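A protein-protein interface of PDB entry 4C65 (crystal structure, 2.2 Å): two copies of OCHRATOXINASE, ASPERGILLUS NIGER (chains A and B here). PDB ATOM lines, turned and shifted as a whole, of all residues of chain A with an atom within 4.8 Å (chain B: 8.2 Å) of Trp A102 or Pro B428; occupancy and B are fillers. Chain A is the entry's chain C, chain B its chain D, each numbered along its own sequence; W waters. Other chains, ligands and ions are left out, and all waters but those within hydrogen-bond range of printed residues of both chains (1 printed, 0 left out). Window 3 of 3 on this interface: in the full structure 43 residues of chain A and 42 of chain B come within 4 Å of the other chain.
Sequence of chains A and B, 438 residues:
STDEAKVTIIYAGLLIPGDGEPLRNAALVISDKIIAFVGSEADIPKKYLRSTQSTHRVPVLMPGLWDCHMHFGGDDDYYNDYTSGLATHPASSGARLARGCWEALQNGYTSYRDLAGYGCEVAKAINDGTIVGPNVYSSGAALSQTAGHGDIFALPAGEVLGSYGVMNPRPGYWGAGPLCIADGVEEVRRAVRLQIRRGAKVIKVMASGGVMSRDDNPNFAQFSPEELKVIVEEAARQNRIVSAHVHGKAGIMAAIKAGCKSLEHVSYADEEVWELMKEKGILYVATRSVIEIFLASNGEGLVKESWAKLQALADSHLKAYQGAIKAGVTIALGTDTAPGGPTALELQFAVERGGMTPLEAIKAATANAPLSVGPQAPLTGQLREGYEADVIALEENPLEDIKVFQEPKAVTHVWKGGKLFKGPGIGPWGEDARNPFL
Of chain B, only Pro B428 and Trp B429 come within 4 Å of Trp A102. Of the printed residues of chain B, Glu A103 touches Asn B435. Gln A106 touches none of the printed residues of chain B. Printed residues of chain A within 4 Å of Trp B102: Pro A428 and Trp A429. Lys B422 touches none of the printed residues of chain A. Pro B428 touches just these residues of chain A: Trp A102 and Pro A428. Of the printed residues of chain A, Asn B435 touches Glu A103 (3.0 Å). Of the printed residues of chain A, Pro B436 touches Arg A99 (3.7 Å). The nearest printed residue of chain A that does not touch Pro B436 is Glu A103 (4.5 Å).
Water W1 lies within hydrogen-bond range of NH2 of Arg A99 (2.7 Å) and O of Arg B434 (2.9 Å).
The backbone carbonyl oxygen of Arg B434 sits at hydrogen-bond distance from the guanidinium group of Arg A99, 3.4 Å away.
Hydrophobic or aromatic side chains of chain B within 4 Å of the printed part of chain A: Trp B102, Ile B131, Pro B428, Trp B429, Pro B436 and Phe B437. Of the 12 printed residues of chain A, 6 touch a printed residue of chain B. Printed residues of chain A that touch a printed residue of chain B: Arg A99, Gly A100, Trp A102, Glu A103, Pro A428 and Trp A429. Hydrophobic or aromatic side chains of chain A within 4 Å of the printed part of chain B: Trp A102, Pro A428 and Trp A429. Among the printed residues, no Asp or Glu carboxylate lies within 4 Å of a Lys or Arg side-chain nitrogen of the other chain.
Ile B131 touches Arg A99. Arg A99 touches Trp B429. Pro B436 touches Arg A99. CE2 of Phe B437 touches CG of Arg A99, at 3.9 Å. CE2 of Phe B437 touches N of Gly A100, 3.5 Å away. Pro B428 touches Trp A102 (CG to CZ2, 3.7 Å). CE3 of Trp A102 touches NE1 of Trp B429, at 3.1 Å. Pro A428 touches Trp B102 (CG to CZ2, 3.7 Å). Pro A428 touches Pro B428 (CB to CB, 3.8 Å). Trp B102 touches Trp A429.
Arg A99 touches Trp B429, and with the chains exchanged Trp A429 touches Arg B99. Trp A102 touches Pro B428, and with the chains exchanged Pro A428 touches Trp B102. Trp A102 touches Trp B429, and with the chains exchanged Trp A429 touches Trp B102. Pro B428 touches its own counterpart, Pro A428. Positions printed for both chains: 99, 102, 103, 105, 106, 132, 428 and 429. Of the 13 pairs that touch across the chains among the printed residues, 7 have their exchanged pair printed and touching as well.
The side-chain carboxylate (OE2) of Glu B103 lies within salt-bridge range of the guanidinium group (NE) of Arg B99 (2.9 Å). O of Pro A428 is in hydrogen-bond range of NE1 of Trp A102, at 2.8 Å. NE of Arg A99 is in salt-bridge range of OE1 of Glu A103 (2.8 Å). OD1 of Asn B435 lies within hydrogen-bond range of N of Phe B437 (2.8 Å). The indole nitrogen (NE1) of Trp B102 is in hydrogen-bond range of the backbone carbonyl oxygen (O) of Pro B428 (2.8 Å).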
ATOM      1  N   ALA A  98     -10.281 -18.662  -8.876  1.00  0.00           N
ATOM      2  CA  ALA A  98     -10.696 -17.274  -9.004  1.00  0.00           C
ATOM      3  C   ALA A  98      -9.477 -16.364  -9.087  1.00  0.00           C
ATOM      4  O   ALA A  98      -9.450 -15.452  -9.891  1.00  0.00           O
ATOM      5  CB  ALA A  98     -11.592 -16.874  -7.831  1.00  0.00           C
ATOM      6  N   ARG A  99      -8.497 -16.592  -8.212  1.00  0.00           N
ATOM      7  CA  ARG A  99      -7.223 -15.893  -8.268  1.00  0.00           C
ATOM      8  C   ARG A  99      -6.564 -16.145  -9.607  1.00  0.00           C
ATOM      9  O   ARG A  99      -6.114 -15.224 -10.261  1.00  0.00           O
ATOM     10  CB  ARG A  99      -6.277 -16.341  -7.148  1.00  0.00           C
ATOM     11  CG  ARG A  99      -4.896 -15.686  -7.195  1.00  0.00           C
ATOM     12  CD  ARG A  99      -5.006 -14.194  -6.872  1.00  0.00           C
ATOM     13  NE  ARG A  99      -3.729 -13.492  -6.776  1.00  0.00           N
ATOM     14  CZ  ARG A  99      -2.919 -13.502  -5.723  1.00  0.00           C
ATOM     15  NH1 ARG A  99      -3.207 -14.202  -4.648  1.00  0.00           N
ATOM     16  NH2 ARG A  99      -1.797 -12.790  -5.762  1.00  0.00           N
ATOM     17  N   GLY A 100      -6.498 -17.410  -9.998  1.00  0.00           N
ATOM     18  CA  GLY A 100      -5.889 -17.812 -11.271  1.00  0.00           C
ATOM     19  C   GLY A 100      -6.478 -17.101 -12.460  1.00  0.00           C
ATOM     20  O   GLY A 100      -5.755 -16.577 -13.289  1.00  0.00           O
ATOM     21  N   CYS A 101      -7.799 -17.037 -12.507  1.00  0.00           N
ATOM     22  CA  CYS A 101      -8.497 -16.338 -13.566  1.00  0.00           C
ATOM     23  C   CYS A 101      -8.232 -14.832 -13.554  1.00  0.00           C
ATOM     24  O   CYS A 101      -8.136 -14.210 -14.630  1.00  0.00           O
ATOM     25  CB  CYS A 101      -9.981 -16.626 -13.480  1.00  0.00           C
ATOM     26  SG  CYS A 101     -10.354 -18.306 -14.015  1.00  0.00           S
ATOM     27  N   TRP A 102      -8.130 -14.243 -12.363  1.00  0.00           N
ATOM     28  CA  TRP A 102      -7.815 -12.827 -12.253  1.00  0.00           C
ATOM     29  C   TRP A 102      -6.454 -12.554 -12.837  1.00  0.00           C
ATOM     30  O   TRP A 102      -6.254 -11.628 -13.603  1.00  0.00           O
ATOM     31  CB  TRP A 102      -7.849 -12.391 -10.787  1.00  0.00           C
ATOM     32  CG  TRP A 102      -7.629 -10.942 -10.598  1.00  0.00           C
ATOM     33  CD1 TRP A 102      -8.576  -9.957 -10.653  1.00  0.00           C
ATOM     34  CD2 TRP A 102      -6.372 -10.283 -10.416  1.00  0.00           C
ATOM     35  NE1 TRP A 102      -7.985  -8.735 -10.502  1.00  0.00           N
ATOM     36  CE2 TRP A 102      -6.633  -8.909 -10.349  1.00  0.00           C
ATOM     37  CE3 TRP A 102      -5.052 -10.732 -10.280  1.00  0.00           C
ATOM     38  CZ2 TRP A 102      -5.642  -7.982 -10.121  1.00  0.00           C
ATOM     39  CZ3 TRP A 102      -4.055  -9.809 -10.065  1.00  0.00           C
ATOM     40  CH2 TRP A 102      -4.350  -8.445  -9.976  1.00  0.00           C
ATOM     41  N   GLU A 103      -5.516 -13.406 -12.468  1.00  0.00           N
ATOM     42  CA  GLU A 103      -4.136 -13.271 -12.866  1.00  0.00           C
ATOM     43  C   GLU A 103      -4.021 -13.429 -14.393  1.00  0.00           C
ATOM     44  O   GLU A 103      -3.303 -12.688 -15.064  1.00  0.00           O
ATOM     45  CB  GLU A 103      -3.292 -14.327 -12.140  1.00  0.00           C
ATOM     46  CG  GLU A 103      -2.023 -13.852 -11.474  1.00  0.00           C
ATOM     47  CD  GLU A 103      -2.084 -12.793 -10.420  1.00  0.00           C
ATOM     48  OE1 GLU A 103      -2.675 -13.014  -9.366  1.00  0.00           O
ATOM     49  OE2 GLU A 103      -1.410 -11.766 -10.633  1.00  0.00           O
ATOM     50  N   ALA A 104      -4.754 -14.397 -14.944  1.00  0.00           N
ATOM     51  CA  ALA A 104      -4.747 -14.632 -16.387  1.00  0.00           C
ATOM     52  C   ALA A 104      -5.129 -13.384 -17.164  1.00  0.00           C
ATOM     53  O   ALA A 104      -4.480 -13.010 -18.140  1.00  0.00           O
ATOM     54  CB  ALA A 104      -5.710 -15.747 -16.747  1.00  0.00           C
ATOM     55  N   LEU A 105      -6.200 -12.747 -16.719  1.00  0.00           N
ATOM     56  CA  LEU A 105      -6.741 -11.588 -17.407  1.00  0.00           C
ATOM     57  C   LEU A 105      -5.796 -10.385 -17.287  1.00  0.00           C
ATOM     58  O   LEU A 105      -5.616  -9.646 -18.248  1.00  0.00           O
ATOM     59  CB  LEU A 105      -8.121 -11.267 -16.831  1.00  0.00           C
ATOM     60  CG  LEU A 105      -9.113 -10.521 -17.722  1.00  0.00           C
ATOM     61  CD1 LEU A 105      -9.321 -11.224 -19.070  1.00  0.00           C
ATOM     62  CD2 LEU A 105     -10.417 -10.379 -16.968  1.00  0.00           C
ATOM     63  N   GLN A 106      -5.158 -10.230 -16.130  1.00  0.00           N
ATOM     64  CA  GLN A 106      -4.165  -9.192 -15.926  1.00  0.00           C
ATOM     65  C   GLN A 106      -2.939  -9.378 -16.799  1.00  0.00           C
ATOM     66  O   GLN A 106      -2.186  -8.429 -17.014  1.00  0.00           O
ATOM     67  CB  GLN A 106      -3.726  -9.156 -14.464  1.00  0.00           C
ATOM     68  CG  GLN A 106      -4.846  -8.789 -13.501  1.00  0.00           C
ATOM     69  CD  GLN A 106      -5.138  -7.306 -13.499  1.00  0.00           C
ATOM     70  OE1 GLN A 106      -4.236  -6.477 -13.314  1.00  0.00           O
ATOM     71  NE2 GLN A 106      -6.399  -6.961 -13.678  1.00  0.00           N
ATOM     72  N   VAL A 132     -13.789 -12.237 -12.262  1.00  0.00           N
ATOM     73  CA  VAL A 132     -13.357 -11.941 -13.597  1.00  0.00           C
ATOM     74  C   VAL A 132     -12.435 -13.021 -14.093  1.00  0.00           C
ATOM     75  O   VAL A 132     -11.810 -13.743 -13.317  1.00  0.00           O
ATOM     76  CB  VAL A 132     -12.673 -10.561 -13.703  1.00  0.00           C
ATOM     77  CG1 VAL A 132     -13.618  -9.461 -13.238  1.00  0.00           C
ATOM     78  CG2 VAL A 132     -11.358 -10.518 -12.951  1.00  0.00           C
ATOM     79  N   PRO A 428      -9.285  -3.470  -9.603  1.00  0.00           N
ATOM     80  CA  PRO A 428      -8.975  -4.865  -9.778  1.00  0.00           C
ATOM     81  C   PRO A 428     -10.063  -5.676 -10.491  1.00  0.00           C
ATOM     82  O   PRO A 428      -9.739  -6.653 -11.158  1.00  0.00           O
ATOM     83  CB  PRO A 428      -8.785  -5.386  -8.346  1.00  0.00           C
ATOM     84  CG  PRO A 428      -9.095  -4.283  -7.416  1.00  0.00           C
ATOM     85  CD  PRO A 428      -9.305  -3.036  -8.196  1.00  0.00           C
ATOM     86  N   TRP A 429     -11.329  -5.302 -10.327  1.00  0.00           N
ATOM     87  CA  TRP A 429     -12.413  -6.095 -10.885  1.00  0.00           C
ATOM     88  C   TRP A 429     -12.961  -5.485 -12.163  1.00  0.00           C
ATOM     89  O   TRP A 429     -13.980  -5.917 -12.660  1.00  0.00           O
ATOM     90  CB  TRP A 429     -13.492  -6.361  -9.838  1.00  0.00           C
ATOM     91  CG  TRP A 429     -12.898  -7.029  -8.633  1.00  0.00           C
ATOM     92  CD1 TRP A 429     -12.573  -6.424  -7.448  1.00  0.00           C
ATOM     93  CD2 TRP A 429     -12.500  -8.403  -8.497  1.00  0.00           C
ATOM     94  NE1 TRP A 429     -12.019  -7.336  -6.588  1.00  0.00           N
ATOM     95  CE2 TRP A 429     -11.957  -8.557  -7.204  1.00  0.00           C
ATOM     96  CE3 TRP A 429     -12.576  -9.518  -9.321  1.00  0.00           C
ATOM     97  CZ2 TRP A 429     -11.495  -9.778  -6.727  1.00  0.00           C
ATOM     98  CZ3 TRP A 429     -12.103 -10.716  -8.855  1.00  0.00           C
ATOM     99  CH2 TRP A 429     -11.577 -10.840  -7.569  1.00  0.00           C
ATOM    100  N   ARG B  99     -14.281 -13.656  -4.280  1.00  0.00           N
ATOM    101  CA  ARG B  99     -14.648 -12.240  -4.401  1.00  0.00           C
ATOM    102  C   ARG B  99     -15.187 -11.699  -3.075  1.00  0.00           C
ATOM    103  O   ARG B  99     -14.758 -10.660  -2.608  1.00  0.00           O
ATOM    104  CB  ARG B  99     -15.687 -12.038  -5.484  1.00  0.00           C
ATOM    105  CG  ARG B  99     -16.153 -10.600  -5.639  1.00  0.00           C
ATOM    106  CD  ARG B  99     -15.032  -9.727  -6.177  1.00  0.00           C
ATOM    107  NE  ARG B  99     -15.455  -8.359  -6.455  1.00  0.00           N
ATOM    108  CZ  ARG B  99     -16.055  -7.967  -7.579  1.00  0.00           C
ATOM    109  NH1 ARG B  99     -16.361  -8.837  -8.539  1.00  0.00           N
ATOM    110  NH2 ARG B  99     -16.388  -6.688  -7.732  1.00  0.00           N
ATOM    111  N   TRP B 102     -12.495 -11.137  -0.566  1.00  0.00           N
ATOM    112  CA  TRP B 102     -11.694  -9.984  -0.937  1.00  0.00           C
ATOM    113  C   TRP B 102     -12.407  -8.718  -0.492  1.00  0.00           C
ATOM    114  O   TRP B 102     -11.791  -7.815   0.094  1.00  0.00           O
ATOM    115  CB  TRP B 102     -11.460  -9.950  -2.443  1.00  0.00           C
ATOM    116  CG  TRP B 102     -10.564  -8.850  -2.876  1.00  0.00           C
ATOM    117  CD1 TRP B 102      -9.207  -8.879  -2.930  1.00  0.00           C
ATOM    118  CD2 TRP B 102     -10.957  -7.527  -3.269  1.00  0.00           C
ATOM    119  NE1 TRP B 102      -8.729  -7.652  -3.341  1.00  0.00           N
ATOM    120  CE2 TRP B 102      -9.792  -6.810  -3.554  1.00  0.00           C
ATOM    121  CE3 TRP B 102     -12.187  -6.887  -3.414  1.00  0.00           C
ATOM    122  CZ2 TRP B 102      -9.825  -5.502  -3.999  1.00  0.00           C
ATOM    123  CZ3 TRP B 102     -12.216  -5.584  -3.846  1.00  0.00           C
ATOM    124  CH2 TRP B 102     -11.052  -4.906  -4.135  1.00  0.00           C
ATOM    125  N   GLU B 103     -13.708  -8.657  -0.771  1.00  0.00           N
ATOM    126  CA  GLU B 103     -14.494  -7.485  -0.486  1.00  0.00           C
ATOM    127  C   GLU B 103     -14.564  -7.263   1.024  1.00  0.00           C
ATOM    128  O   GLU B 103     -14.465  -6.141   1.506  1.00  0.00           O
ATOM    129  CB  GLU B 103     -15.896  -7.669  -1.053  1.00  0.00           C
ATOM    130  CG  GLU B 103     -16.078  -7.622  -2.561  1.00  0.00           C
ATOM    131  CD  GLU B 103     -15.708  -6.304  -3.219  1.00  0.00           C
ATOM    132  OE1 GLU B 103     -15.742  -5.258  -2.555  1.00  0.00           O
ATOM    133  OE2 GLU B 103     -15.388  -6.279  -4.446  1.00  0.00           O
ATOM    134  N   LEU B 105     -12.398  -8.005   3.327  1.00  0.00           N
ATOM    135  CA  LEU B 105     -11.138  -7.529   3.860  1.00  0.00           C
ATOM    136  C   LEU B 105     -10.920  -6.067   3.488  1.00  0.00           C
ATOM    137  O   LEU B 105     -10.425  -5.287   4.291  1.00  0.00           O
ATOM    138  CB  LEU B 105     -10.005  -8.414   3.341  1.00  0.00           C
ATOM    139  CG  LEU B 105      -8.715  -8.512   4.139  1.00  0.00           C
ATOM    140  CD1 LEU B 105      -8.979  -8.911   5.583  1.00  0.00           C
ATOM    141  CD2 LEU B 105      -7.779  -9.494   3.457  1.00  0.00           C
ATOM    142  N   GLN B 106     -11.319  -5.695   2.280  1.00  0.00           N
ATOM    143  CA  GLN B 106     -11.258  -4.307   1.838  1.00  0.00           C
ATOM    144  C   GLN B 106     -12.162  -3.395   2.648  1.00  0.00           C
ATOM    145  O   GLN B 106     -11.965  -2.173   2.657  1.00  0.00           O
ATOM    146  CB  GLN B 106     -11.654  -4.193   0.359  1.00  0.00           C
ATOM    147  CG  GLN B 106     -10.704  -4.911  -0.570  1.00  0.00           C
ATOM    148  CD  GLN B 106      -9.439  -4.139  -0.821  1.00  0.00           C
ATOM    149  OE1 GLN B 106      -9.463  -2.956  -1.192  1.00  0.00           O
ATOM    150  NE2 GLN B 106      -8.306  -4.798  -0.622  1.00  0.00           N
ATOM    151  N   ILE B 131      -5.698 -16.838  -2.176  1.00  0.00           N
ATOM    152  CA  ILE B 131      -6.596 -15.708  -2.148  1.00  0.00           C
ATOM    153  C   ILE B 131      -6.422 -14.997  -0.833  1.00  0.00           C
ATOM    154  O   ILE B 131      -5.638 -15.416   0.016  1.00  0.00           O
ATOM    155  CB  ILE B 131      -8.077 -16.095  -2.373  1.00  0.00           C
ATOM    156  CG1 ILE B 131      -8.579 -17.026  -1.279  1.00  0.00           C
ATOM    157  CG2 ILE B 131      -8.282 -16.734  -3.744  1.00  0.00           C
ATOM    158  CD1 ILE B 131     -10.085 -17.093  -1.210  1.00  0.00           C
ATOM    159  N   VAL B 132      -7.166 -13.922  -0.660  1.00  0.00           N
ATOM    160  CA  VAL B 132      -7.142 -13.192   0.593  1.00  0.00           C
ATOM    161  C   VAL B 132      -8.536 -13.163   1.211  1.00  0.00           C
ATOM    162  O   VAL B 132      -9.556 -13.314   0.529  1.00  0.00           O
ATOM    163  CB  VAL B 132      -6.598 -11.764   0.417  1.00  0.00           C
ATOM    164  CG1 VAL B 132      -5.197 -11.803  -0.165  1.00  0.00           C
ATOM    165  CG2 VAL B 132      -7.538 -10.894  -0.417  1.00  0.00           C
ATOM    166  N   GLY B 133      -8.579 -12.942   2.507  1.00  0.00           N
ATOM    167  CA  GLY B 133      -9.847 -12.803   3.183  1.00  0.00           C
ATOM    168  C   GLY B 133      -9.665 -12.647   4.669  1.00  0.00           C
ATOM    169  O   GLY B 133      -8.548 -12.633   5.157  1.00  0.00           O
ATOM    170  N   LEU B 420      -0.155  -6.179   5.748  1.00  0.00           N
ATOM    171  CA  LEU B 420      -0.983  -5.135   5.181  1.00  0.00           C
ATOM    172  C   LEU B 420      -1.642  -5.650   3.897  1.00  0.00           C
ATOM    173  O   LEU B 420      -0.968  -5.940   2.919  1.00  0.00           O
ATOM    174  CB  LEU B 420      -0.100  -3.934   4.879  1.00  0.00           C
ATOM    175  CG  LEU B 420      -0.687  -2.538   4.680  1.00  0.00           C
ATOM    176  CD1 LEU B 420      -1.600  -2.147   5.819  1.00  0.00           C
ATOM    177  CD2 LEU B 420       0.412  -1.497   4.515  1.00  0.00           C
ATOM    178  N   PHE B 421      -2.965  -5.771   3.921  1.00  0.00           N
ATOM    179  CA  PHE B 421      -3.747  -6.221   2.783  1.00  0.00           C
ATOM    180  C   PHE B 421      -4.437  -5.089   2.014  1.00  0.00           C
ATOM    181  O   PHE B 421      -4.883  -5.277   0.878  1.00  0.00           O
ATOM    182  CB  PHE B 421      -4.760  -7.278   3.234  1.00  0.00           C
ATOM    183  CG  PHE B 421      -4.126  -8.603   3.526  1.00  0.00           C
ATOM    184  CD1 PHE B 421      -3.816  -9.474   2.488  1.00  0.00           C
ATOM    185  CD2 PHE B 421      -3.840  -8.995   4.827  1.00  0.00           C
ATOM    186  CE1 PHE B 421      -3.238 -10.711   2.747  1.00  0.00           C
ATOM    187  CE2 PHE B 421      -3.245 -10.215   5.083  1.00  0.00           C
ATOM    188  CZ  PHE B 421      -2.936 -11.069   4.045  1.00  0.00           C
ATOM    189  N   LYS B 422      -4.530  -3.929   2.646  1.00  0.00           N
ATOM    190  CA  LYS B 422      -5.039  -2.728   2.007  1.00  0.00           C
ATOM    191  C   LYS B 422      -4.277  -1.525   2.553  1.00  0.00           C
ATOM    192  O   LYS B 422      -4.021  -1.441   3.750  1.00  0.00           O
ATOM    193  CB  LYS B 422      -6.547  -2.561   2.272  1.00  0.00           C
ATOM    194  CG  LYS B 422      -7.219  -1.441   1.468  1.00  0.00           C
ATOM    195  CD  LYS B 422      -8.616  -1.157   1.979  1.00  0.00           C
ATOM    196  CE  LYS B 422      -9.356  -0.213   1.053  1.00  0.00           C
ATOM    197  NZ  LYS B 422     -10.733   0.073   1.541  1.00  0.00           N
ATOM    198  N   GLY B 423      -3.935  -0.603   1.665  1.00  0.00           N
ATOM    199  CA  GLY B 423      -3.241   0.616   2.048  1.00  0.00           C
ATOM    200  C   GLY B 423      -2.741   1.368   0.844  1.00  0.00           C
ATOM    201  O   GLY B 423      -2.703   0.815  -0.241  1.00  0.00           O
ATOM    202  N   GLY B 425      -0.731   2.545  -2.089  1.00  0.00           N
ATOM    203  CA  GLY B 425       0.338   1.844  -2.817  1.00  0.00           C
ATOM    204  C   GLY B 425       0.292   0.325  -2.788  1.00  0.00           C
ATOM    205  O   GLY B 425       1.122  -0.318  -3.415  1.00  0.00           O
ATOM    206  N   ILE B 426      -0.678  -0.257  -2.076  1.00  0.00           N
ATOM    207  CA  ILE B 426      -0.739  -1.712  -1.905  1.00  0.00           C
ATOM    208  C   ILE B 426      -1.756  -2.315  -2.882  1.00  0.00           C
ATOM    209  O   ILE B 426      -2.910  -1.895  -2.946  1.00  0.00           O
ATOM    210  CB  ILE B 426      -1.079  -2.100  -0.440  1.00  0.00           C
ATOM    211  CG1 ILE B 426      -0.077  -1.504   0.568  1.00  0.00           C
ATOM    212  CG2 ILE B 426      -1.381  -3.597  -0.345  1.00  0.00           C
ATOM    213  CD1 ILE B 426       1.394  -1.833   0.415  1.00  0.00           C
ATOM    214  N   GLY B 427      -1.303  -3.295  -3.662  1.00  0.00           N
ATOM    215  CA  GLY B 427      -2.119  -3.916  -4.693  1.00  0.00           C
ATOM    216  C   GLY B 427      -3.271  -4.743  -4.144  1.00  0.00           C
ATOM    217  O   GLY B 427      -3.420  -4.904  -2.934  1.00  0.00           O
ATOM    218  N   PRO B 428      -4.098  -5.284  -5.049  1.00  0.00           N
ATOM    219  CA  PRO B 428      -5.340  -5.930  -4.656  1.00  0.00           C
ATOM    220  C   PRO B 428      -5.133  -7.139  -3.749  1.00  0.00           C
ATOM    221  O   PRO B 428      -5.994  -7.431  -2.929  1.00  0.00           O
ATOM    222  CB  PRO B 428      -5.963  -6.353  -5.980  1.00  0.00           C
ATOM    223  CG  PRO B 428      -5.021  -5.987  -7.065  1.00  0.00           C
ATOM    224  CD  PRO B 428      -3.908  -5.199  -6.507  1.00  0.00           C
ATOM    225  N   TRP B 429      -4.011  -7.828  -3.889  1.00  0.00           N
ATOM    226  CA  TRP B 429      -3.792  -9.045  -3.116  1.00  0.00           C
ATOM    227  C   TRP B 429      -2.872  -8.845  -1.920  1.00  0.00           C
ATOM    228  O   TRP B 429      -2.432  -9.788  -1.314  1.00  0.00           O
ATOM    229  CB  TRP B 429      -3.323 -10.169  -4.046  1.00  0.00           C
ATOM    230  CG  TRP B 429      -4.312 -10.376  -5.167  1.00  0.00           C
ATOM    231  CD1 TRP B 429      -4.195  -9.926  -6.441  1.00  0.00           C
ATOM    232  CD2 TRP B 429      -5.586 -11.024  -5.086  1.00  0.00           C
ATOM    233  NE1 TRP B 429      -5.303 -10.282  -7.178  1.00  0.00           N
ATOM    234  CE2 TRP B 429      -6.169 -10.968  -6.378  1.00  0.00           C
ATOM    235  CE3 TRP B 429      -6.285 -11.667  -4.059  1.00  0.00           C
ATOM    236  CZ2 TRP B 429      -7.417 -11.525  -6.669  1.00  0.00           C
ATOM    237  CZ3 TRP B 429      -7.532 -12.220  -4.344  1.00  0.00           C
ATOM    238  CH2 TRP B 429      -8.090 -12.129  -5.631  1.00  0.00           C
ATOM    239  N   GLY B 430      -2.609  -7.595  -1.579  1.00  0.00           N
ATOM    240  CA  GLY B 430      -1.828  -7.270  -0.386  1.00  0.00           C
ATOM    241  C   GLY B 430      -0.348  -7.048  -0.646  1.00  0.00           C
ATOM    242  O   GLY B 430       0.133  -7.308  -1.738  1.00  0.00           O
ATOM    243  N   GLU B 431       0.366  -6.586   0.381  1.00  0.00           N
ATOM    244  CA  GLU B 431       1.770  -6.238   0.232  1.00  0.00           C
ATOM    245  C   GLU B 431       2.594  -7.442  -0.166  1.00  0.00           C
ATOM    246  O   GLU B 431       2.329  -8.569   0.295  1.00  0.00           O
ATOM    247  CB  GLU B 431       2.366  -5.610   1.489  1.00  0.00           C
ATOM    248  CG  GLU B 431       2.419  -6.516   2.705  1.00  0.00           C
ATOM    249  CD  GLU B 431       3.040  -5.836   3.918  1.00  0.00           C
ATOM    250  OE1 GLU B 431       3.875  -4.898   3.746  1.00  0.00           O
ATOM    251  OE2 GLU B 431       2.708  -6.269   5.054  1.00  0.00           O
ATOM    252  N   ALA B 433       2.526  -9.149  -2.766  1.00  0.00           N
ATOM    253  CA  ALA B 433       1.763 -10.220  -3.371  1.00  0.00           C
ATOM    254  C   ALA B 433       2.550 -10.671  -4.572  1.00  0.00           C
ATOM    255  O   ALA B 433       3.160  -9.873  -5.264  1.00  0.00           O
ATOM    256  CB  ALA B 433       0.363  -9.759  -3.766  1.00  0.00           C
ATOM    257  N   ARG B 434       2.551 -11.976  -4.783  1.00  0.00           N
ATOM    258  CA  ARG B 434       3.141 -12.584  -5.960  1.00  0.00           C
ATOM    259  C   ARG B 434       2.089 -13.530  -6.519  1.00  0.00           C
ATOM    260  O   ARG B 434       1.311 -14.100  -5.783  1.00  0.00           O
ATOM    261  CB  ARG B 434       4.420 -13.352  -5.587  1.00  0.00           C
ATOM    262  CG  ARG B 434       5.724 -12.569  -5.405  1.00  0.00           C
ATOM    263  CD  ARG B 434       6.926 -13.516  -5.495  1.00  0.00           C
ATOM    264  NE  ARG B 434       7.411 -13.655  -6.902  1.00  0.00           N
ATOM    265  CZ  ARG B 434       6.970 -14.540  -7.832  1.00  0.00           C
ATOM    266  NH1 ARG B 434       6.035 -15.455  -7.554  1.00  0.00           N
ATOM    267  NH2 ARG B 434       7.482 -14.518  -9.062  1.00  0.00           N
ATOM    268  N   ASN B 435       2.065 -13.691  -7.828  1.00  0.00           N
ATOM    269  CA  ASN B 435       1.195 -14.669  -8.453  1.00  0.00           C
ATOM    270  C   ASN B 435       1.562 -16.053  -7.911  1.00  0.00           C
ATOM    271  O   ASN B 435       2.631 -16.588  -8.233  1.00  0.00           O
ATOM    272  CB  ASN B 435       1.352 -14.605  -9.985  1.00  0.00           C
ATOM    273  CG  ASN B 435       0.492 -15.622 -10.715  1.00  0.00           C
ATOM    274  OD1 ASN B 435      -0.144 -16.473 -10.104  1.00  0.00           O
ATOM    275  ND2 ASN B 435       0.444 -15.507 -12.026  1.00  0.00           N
ATOM    276  N   PRO B 436       0.673 -16.652  -7.111  1.00  0.00           N
ATOM    277  CA  PRO B 436       0.977 -17.983  -6.592  1.00  0.00           C
ATOM    278  C   PRO B 436       1.073 -19.124  -7.619  1.00  0.00           C
ATOM    279  O   PRO B 436       1.452 -20.217  -7.226  1.00  0.00           O
ATOM    280  CB  PRO B 436      -0.181 -18.275  -5.647  1.00  0.00           C
ATOM    281  CG  PRO B 436      -1.309 -17.459  -6.164  1.00  0.00           C
ATOM    282  CD  PRO B 436      -0.713 -16.251  -6.846  1.00  0.00           C
ATOM    283  N   PHE B 437       0.737 -18.893  -8.887  1.00  0.00           N
ATOM    284  CA  PHE B 437       0.712 -19.966  -9.877  1.00  0.00           C
ATOM    285  C   PHE B 437       1.948 -19.963 -10.753  1.00  0.00           C
ATOM    286  O   PHE B 437       2.034 -20.721 -11.717  1.00  0.00           O
ATOM    287  CB  PHE B 437      -0.586 -19.876 -10.701  1.00  0.00           C
ATOM    288  CG  PHE B 437      -1.832 -20.031  -9.859  1.00  0.00           C
ATOM    289  CD1 PHE B 437      -2.193 -21.272  -9.357  1.00  0.00           C
ATOM    290  CD2 PHE B 437      -2.620 -18.942  -9.547  1.00  0.00           C
ATOM    291  CE1 PHE B 437      -3.320 -21.421  -8.570  1.00  0.00           C
ATOM    292  CE2 PHE B 437      -3.741 -19.078  -8.752  1.00  0.00           C
ATOM    293  CZ  PHE B 437      -4.096 -20.318  -8.266  1.00  0.00           C
HETATM  294  O   HOH W   1      -0.200 -12.823  -3.597  1.00  0.00           O
